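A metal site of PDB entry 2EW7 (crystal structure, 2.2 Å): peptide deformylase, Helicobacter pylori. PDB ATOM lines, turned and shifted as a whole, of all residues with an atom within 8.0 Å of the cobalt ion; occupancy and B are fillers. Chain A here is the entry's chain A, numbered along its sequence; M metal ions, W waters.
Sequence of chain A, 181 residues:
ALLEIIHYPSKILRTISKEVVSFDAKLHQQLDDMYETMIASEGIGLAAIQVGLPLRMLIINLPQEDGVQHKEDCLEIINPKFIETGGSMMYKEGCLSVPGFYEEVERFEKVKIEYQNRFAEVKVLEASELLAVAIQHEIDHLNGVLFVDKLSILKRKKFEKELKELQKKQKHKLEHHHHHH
OE1 of Glu 93 lies within hydrogen-bond range of ND1 of His 137 (2.7 Å).
SG of Cys 95 lies close to NE2 of Gln 50 (3.5 Å).
The backbone NH (N) of Ser 97 lies close to the side-chain sulfur (SG) of Cys 95 (3.4 Å).
The side-chain amide nitrogen of Gln 50 sits at hydrogen-bond distance from the side-chain hydroxyl of Ser 97 (3.0 Å).
N of Ala 47 sits at hydrogen-bond distance from OE1 of Gln 50.
OE1 of Glu 138 sits at hydrogen-bond distance from N of Ala 47.
The backbone NH (N) of Leu 46 is in hydrogen-bond range of the side-chain carboxylate (OE2) of Glu 138 (3.5 Å).
Gln 50 touches the cobalt ion.
OE2 of Glu 138 touches the cobalt ion (3.98 Å).
The cobalt ion is bound by NE2 of His 137, 2.2 Å away.
A ring nitrogen (NE2) of His 141 binds the cobalt ion (2.2 Å).
Water W1 is bound to the cobalt ion (2.2 Å).
The side-chain sulfur (SG) of Cys 95 is bound to the cobalt ion (2.4 Å).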
ATOM      1  N   LEU A  13      -2.078  17.571 -29.704  1.00  0.00           N
ATOM      2  CA  LEU A  13      -2.769  17.792 -28.447  1.00  0.00           C
ATOM      3  C   LEU A  13      -4.029  18.667 -28.602  1.00  0.00           C
ATOM      4  O   LEU A  13      -4.816  18.797 -27.662  1.00  0.00           O
ATOM      5  CB  LEU A  13      -1.810  18.415 -27.430  1.00  0.00           C
ATOM      6  CG  LEU A  13      -0.611  17.531 -27.038  1.00  0.00           C
ATOM      7  CD1 LEU A  13       0.346  18.301 -26.135  1.00  0.00           C
ATOM      8  CD2 LEU A  13      -1.111  16.262 -26.336  1.00  0.00           C
ATOM      9  N   GLY A  45      -2.433  10.746 -14.062  1.00  0.00           N
ATOM     10  CA  GLY A  45      -3.486  10.810 -15.060  1.00  0.00           C
ATOM     11  C   GLY A  45      -2.915  10.799 -16.471  1.00  0.00           C
ATOM     12  O   GLY A  45      -1.795  11.252 -16.698  1.00  0.00           O
ATOM     13  N   LEU A  46      -3.684  10.269 -17.425  1.00  0.00           N
ATOM     14  CA  LEU A  46      -3.246  10.222 -18.814  1.00  0.00           C
ATOM     15  C   LEU A  46      -4.412  10.009 -19.781  1.00  0.00           C
ATOM     16  O   LEU A  46      -5.197   9.073 -19.635  1.00  0.00           O
ATOM     17  CB  LEU A  46      -2.221   9.098 -19.011  1.00  0.00           C
ATOM     18  CG  LEU A  46      -1.645   9.006 -20.432  1.00  0.00           C
ATOM     19  CD1 LEU A  46      -0.670  10.166 -20.641  1.00  0.00           C
ATOM     20  CD2 LEU A  46      -0.933   7.666 -20.634  1.00  0.00           C
ATOM     21  N   ALA A  47      -4.522  10.891 -20.772  1.00  0.00           N
ATOM     22  CA  ALA A  47      -5.565  10.795 -21.790  1.00  0.00           C
ATOM     23  C   ALA A  47      -4.979  10.139 -23.021  1.00  0.00           C
ATOM     24  O   ALA A  47      -3.769  10.220 -23.269  1.00  0.00           O
ATOM     25  CB  ALA A  47      -6.087  12.176 -22.129  1.00  0.00           C
ATOM     26  N   ILE A  49      -5.036  10.906 -26.295  1.00  0.00           N
ATOM     27  CA  ILE A  49      -4.278  11.721 -27.264  1.00  0.00           C
ATOM     28  C   ILE A  49      -2.866  12.002 -26.813  1.00  0.00           C
ATOM     29  O   ILE A  49      -2.006  12.328 -27.626  1.00  0.00           O
ATOM     30  CB  ILE A  49      -4.924  13.103 -27.578  1.00  0.00           C
ATOM     31  CG1 ILE A  49      -5.785  13.557 -26.413  1.00  0.00           C
ATOM     32  CG2 ILE A  49      -5.635  13.063 -28.910  1.00  0.00           C
ATOM     33  CD1 ILE A  49      -4.993  14.035 -25.232  1.00  0.00           C
ATOM     34  N   GLN A  50      -2.619  11.897 -25.509  1.00  0.00           N
ATOM     35  CA  GLN A  50      -1.285  12.128 -24.990  1.00  0.00           C
ATOM     36  C   GLN A  50      -0.311  11.071 -25.506  1.00  0.00           C
ATOM     37  O   GLN A  50       0.899  11.219 -25.388  1.00  0.00           O
ATOM     38  CB  GLN A  50      -1.316  12.170 -23.465  1.00  0.00           C
ATOM     39  CG  GLN A  50      -1.892  13.465 -22.906  1.00  0.00           C
ATOM     40  CD  GLN A  50      -1.852  13.528 -21.396  1.00  0.00           C
ATOM     41  OE1 GLN A  50      -2.649  12.877 -20.722  1.00  0.00           O
ATOM     42  NE2 GLN A  50      -0.919  14.296 -20.849  1.00  0.00           N
ATOM     43  N   GLU A  93      -1.799  22.553 -10.880  1.00  0.00           N
ATOM     44  CA  GLU A  93      -1.725  21.354 -11.716  1.00  0.00           C
ATOM     45  C   GLU A  93      -0.431  21.173 -12.506  1.00  0.00           C
ATOM     46  O   GLU A  93       0.341  22.113 -12.713  1.00  0.00           O
ATOM     47  CB  GLU A  93      -2.898  21.353 -12.700  1.00  0.00           C
ATOM     48  CG  GLU A  93      -4.263  21.116 -12.070  1.00  0.00           C
ATOM     49  CD  GLU A  93      -5.396  21.212 -13.076  1.00  0.00           C
ATOM     50  OE1 GLU A  93      -5.204  20.818 -14.248  1.00  0.00           O
ATOM     51  OE2 GLU A  93      -6.496  21.681 -12.704  1.00  0.00           O
ATOM     52  N   GLY A  94      -0.217  19.935 -12.943  1.00  0.00           N
ATOM     53  CA  GLY A  94       0.935  19.584 -13.750  1.00  0.00           C
ATOM     54  C   GLY A  94       0.374  18.748 -14.877  1.00  0.00           C
ATOM     55  O   GLY A  94      -0.831  18.504 -14.916  1.00  0.00           O
ATOM     56  N   CYS A  95       1.223  18.286 -15.797  1.00  0.00           N
ATOM     57  CA  CYS A  95       0.751  17.483 -16.917  1.00  0.00           C
ATOM     58  C   CYS A  95       1.925  16.796 -17.623  1.00  0.00           C
ATOM     59  O   CYS A  95       2.924  17.444 -17.915  1.00  0.00           O
ATOM     60  CB  CYS A  95      -0.003  18.353 -17.930  1.00  0.00           C
ATOM     61  SG  CYS A  95      -0.682  17.449 -19.359  1.00  0.00           S
ATOM     62  N   LEU A  96       1.795  15.504 -17.883  1.00  0.00           N
ATOM     63  CA  LEU A  96       2.857  14.768 -18.562  1.00  0.00           C
ATOM     64  C   LEU A  96       3.165  15.348 -19.942  1.00  0.00           C
ATOM     65  O   LEU A  96       4.263  15.157 -20.470  1.00  0.00           O
ATOM     66  CB  LEU A  96       2.496  13.282 -18.690  1.00  0.00           C
ATOM     67  CG  LEU A  96       2.496  12.518 -17.357  1.00  0.00           C
ATOM     68  CD1 LEU A  96       2.180  11.052 -17.604  1.00  0.00           C
ATOM     69  CD2 LEU A  96       3.846  12.656 -16.692  1.00  0.00           C
ATOM     70  N   SER A  97       2.210  16.060 -20.528  1.00  0.00           N
ATOM     71  CA  SER A  97       2.437  16.663 -21.837  1.00  0.00           C
ATOM     72  C   SER A  97       3.044  18.061 -21.713  1.00  0.00           C
ATOM     73  O   SER A  97       3.339  18.710 -22.715  1.00  0.00           O
ATOM     74  CB  SER A  97       1.126  16.728 -22.633  1.00  0.00           C
ATOM     75  OG  SER A  97       0.747  15.432 -23.071  1.00  0.00           O
ATOM     76  N   VAL A  98       3.225  18.516 -20.483  1.00  0.00           N
ATOM     77  CA  VAL A  98       3.808  19.820 -20.219  1.00  0.00           C
ATOM     78  C   VAL A  98       4.781  19.665 -19.046  1.00  0.00           C
ATOM     79  O   VAL A  98       4.636  20.325 -18.021  1.00  0.00           O
ATOM     80  CB  VAL A  98       2.712  20.848 -19.839  1.00  0.00           C
ATOM     81  CG1 VAL A  98       3.290  22.265 -19.880  1.00  0.00           C
ATOM     82  CG2 VAL A  98       1.533  20.734 -20.808  1.00  0.00           C
ATOM     83  N   ARG A 107     -10.976  25.221 -11.107  1.00  0.00           N
ATOM     84  CA  ARG A 107     -11.730  24.021 -11.410  1.00  0.00           C
ATOM     85  C   ARG A 107     -12.990  23.934 -10.555  1.00  0.00           C
ATOM     86  O   ARG A 107     -13.096  24.589  -9.517  1.00  0.00           O
ATOM     87  CB  ARG A 107     -10.884  22.776 -11.124  1.00  0.00           C
ATOM     88  CG  ARG A 107      -9.628  22.625 -11.945  1.00  0.00           C
ATOM     89  CD  ARG A 107      -9.936  22.245 -13.382  1.00  0.00           C
ATOM     90  NE  ARG A 107      -8.714  22.008 -14.146  1.00  0.00           N
ATOM     91  CZ  ARG A 107      -8.681  21.769 -15.455  1.00  0.00           C
ATOM     92  NH1 ARG A 107      -9.798  21.731 -16.159  1.00  0.00           N
ATOM     93  NH2 ARG A 107      -7.512  21.555 -16.056  1.00  0.00           N
ATOM     94  N   ALA A 134      -8.496  15.832 -11.476  1.00  0.00           N
ATOM     95  CA  ALA A 134      -7.929  14.943 -12.482  1.00  0.00           C
ATOM     96  C   ALA A 134      -8.965  14.660 -13.566  1.00  0.00           C
ATOM     97  O   ALA A 134      -8.656  14.659 -14.756  1.00  0.00           O
ATOM     98  CB  ALA A 134      -7.482  13.634 -11.832  1.00  0.00           C
ATOM     99  N   HIS A 137      -9.280  17.737 -15.746  1.00  0.00           N
ATOM    100  CA  HIS A 137      -8.055  17.907 -16.516  1.00  0.00           C
ATOM    101  C   HIS A 137      -8.000  16.893 -17.655  1.00  0.00           C
ATOM    102  O   HIS A 137      -7.793  17.253 -18.809  1.00  0.00           O
ATOM    103  CB  HIS A 137      -6.858  17.703 -15.572  1.00  0.00           C
ATOM    104  CG  HIS A 137      -5.522  17.833 -16.249  1.00  0.00           C
ATOM    105  ND1 HIS A 137      -4.705  18.929 -16.082  1.00  0.00           N
ATOM    106  CD2 HIS A 137      -4.816  16.961 -17.015  1.00  0.00           C
ATOM    107  CE1 HIS A 137      -3.562  18.737 -16.718  1.00  0.00           C
ATOM    108  NE2 HIS A 137      -3.606  17.546 -17.284  1.00  0.00           N
ATOM    109  N   GLU A 138      -8.198  15.620 -17.330  1.00  0.00           N
ATOM    110  CA  GLU A 138      -8.147  14.600 -18.360  1.00  0.00           C
ATOM    111  C   GLU A 138      -9.238  14.776 -19.416  1.00  0.00           C
ATOM    112  O   GLU A 138      -8.972  14.604 -20.602  1.00  0.00           O
ATOM    113  CB  GLU A 138      -8.228  13.209 -17.735  1.00  0.00           C
ATOM    114  CG  GLU A 138      -7.022  12.835 -16.881  1.00  0.00           C
ATOM    115  CD  GLU A 138      -5.697  13.152 -17.542  1.00  0.00           C
ATOM    116  OE1 GLU A 138      -5.587  13.025 -18.785  1.00  0.00           O
ATOM    117  OE2 GLU A 138      -4.739  13.511 -16.812  1.00  0.00           O
ATOM    118  N   ILE A 139     -10.450  15.128 -18.992  1.00  0.00           N
ATOM    119  CA  ILE A 139     -11.523  15.331 -19.962  1.00  0.00           C
ATOM    120  C   ILE A 139     -11.212  16.507 -20.878  1.00  0.00           C
ATOM    121  O   ILE A 139     -11.581  16.491 -22.059  1.00  0.00           O
ATOM    122  CB  ILE A 139     -12.887  15.507 -19.246  1.00  0.00           C
ATOM    123  CG1 ILE A 139     -13.357  14.139 -18.742  1.00  0.00           C
ATOM    124  CG2 ILE A 139     -13.928  16.098 -20.209  1.00  0.00           C
ATOM    125  CD1 ILE A 139     -14.647  14.180 -17.932  1.00  0.00           C
ATOM    126  N   ASP A 140     -10.517  17.521 -20.370  1.00  0.00           N
ATOM    127  CA  ASP A 140     -10.155  18.659 -21.209  1.00  0.00           C
ATOM    128  C   ASP A 140      -9.263  18.164 -22.364  1.00  0.00           C
ATOM    129  O   ASP A 140      -9.368  18.649 -23.492  1.00  0.00           O
ATOM    130  CB  ASP A 140      -9.381  19.719 -20.394  1.00  0.00           C
ATOM    131  CG  ASP A 140     -10.299  20.760 -19.760  1.00  0.00           C
ATOM    132  OD1 ASP A 140     -11.510  20.769 -20.073  1.00  0.00           O
ATOM    133  OD2 ASP A 140      -9.796  21.576 -18.956  1.00  0.00           O
ATOM    134  N   HIS A 141      -8.399  17.185 -22.077  1.00  0.00           N
ATOM    135  CA  HIS A 141      -7.530  16.621 -23.109  1.00  0.00           C
ATOM    136  C   HIS A 141      -8.331  16.053 -24.272  1.00  0.00           C
ATOM    137  O   HIS A 141      -7.942  16.189 -25.426  1.00  0.00           O
ATOM    138  CB  HIS A 141      -6.648  15.519 -22.536  1.00  0.00           C
ATOM    139  CG  HIS A 141      -5.389  16.020 -21.921  1.00  0.00           C
ATOM    140  ND1 HIS A 141      -4.508  16.838 -22.599  1.00  0.00           N
ATOM    141  CD2 HIS A 141      -4.845  15.826 -20.693  1.00  0.00           C
ATOM    142  CE1 HIS A 141      -3.482  17.120 -21.820  1.00  0.00           C
ATOM    143  NE2 HIS A 141      -3.669  16.519 -20.658  1.00  0.00           N
ATOM    144  N   VAL A 145      -7.900  20.488 -25.063  1.00  0.00           N
ATOM    145  CA  VAL A 145      -7.576  21.567 -24.140  1.00  0.00           C
ATOM    146  C   VAL A 145      -6.478  21.161 -23.145  1.00  0.00           C
ATOM    147  O   VAL A 145      -6.488  20.051 -22.614  1.00  0.00           O
ATOM    148  CB  VAL A 145      -8.822  22.015 -23.345  1.00  0.00           C
ATOM    149  CG1 VAL A 145      -8.444  23.024 -22.268  1.00  0.00           C
ATOM    150  CG2 VAL A 145      -9.855  22.622 -24.295  1.00  0.00           C
ATOM    151  N   LEU A 146      -5.529  22.082 -22.920  1.00  0.00           N
ATOM    152  CA  LEU A 146      -4.421  21.875 -21.988  1.00  0.00           C
ATOM    153  C   LEU A 146      -4.638  22.838 -20.828  1.00  0.00           C
ATOM    154  O   LEU A 146      -5.268  23.876 -20.997  1.00  0.00           O
ATOM    155  CB  LEU A 146      -3.094  22.204 -22.665  1.00  0.00           C
ATOM    156  CG  LEU A 146      -2.740  21.394 -23.922  1.00  0.00           C
ATOM    157  CD1 LEU A 146      -1.435  21.909 -24.499  1.00  0.00           C
ATOM    158  CD2 LEU A 146      -2.651  19.912 -23.563  1.00  0.00           C
ATOM    159  N   PHE A 147      -4.112  22.501 -19.648  1.00  0.00           N
ATOM    160  CA  PHE A 147      -4.343  23.369 -18.498  1.00  0.00           C
ATOM    161  C   PHE A 147      -3.698  24.757 -18.655  1.00  0.00           C
ATOM    162  O   PHE A 147      -4.155  25.719 -18.047  1.00  0.00           O
ATOM    163  CB  PHE A 147      -3.891  22.707 -17.181  1.00  0.00           C
ATOM    164  CG  PHE A 147      -2.399  22.730 -16.942  1.00  0.00           C
ATOM    165  CD1 PHE A 147      -1.558  21.830 -17.578  1.00  0.00           C
ATOM    166  CD2 PHE A 147      -1.854  23.634 -16.028  1.00  0.00           C
ATOM    167  CE1 PHE A 147      -0.190  21.826 -17.308  1.00  0.00           C
ATOM    168  CE2 PHE A 147      -0.487  23.638 -15.753  1.00  0.00           C
ATOM    169  CZ  PHE A 147       0.345  22.730 -16.396  1.00  0.00           C
HETATM  170 CO    CO M   1      -2.668  16.298 -18.765  1.00  0.00          CO
HETATM  171  O   HOH W   1      -2.760  14.157 -18.331  1.00  0.00           O
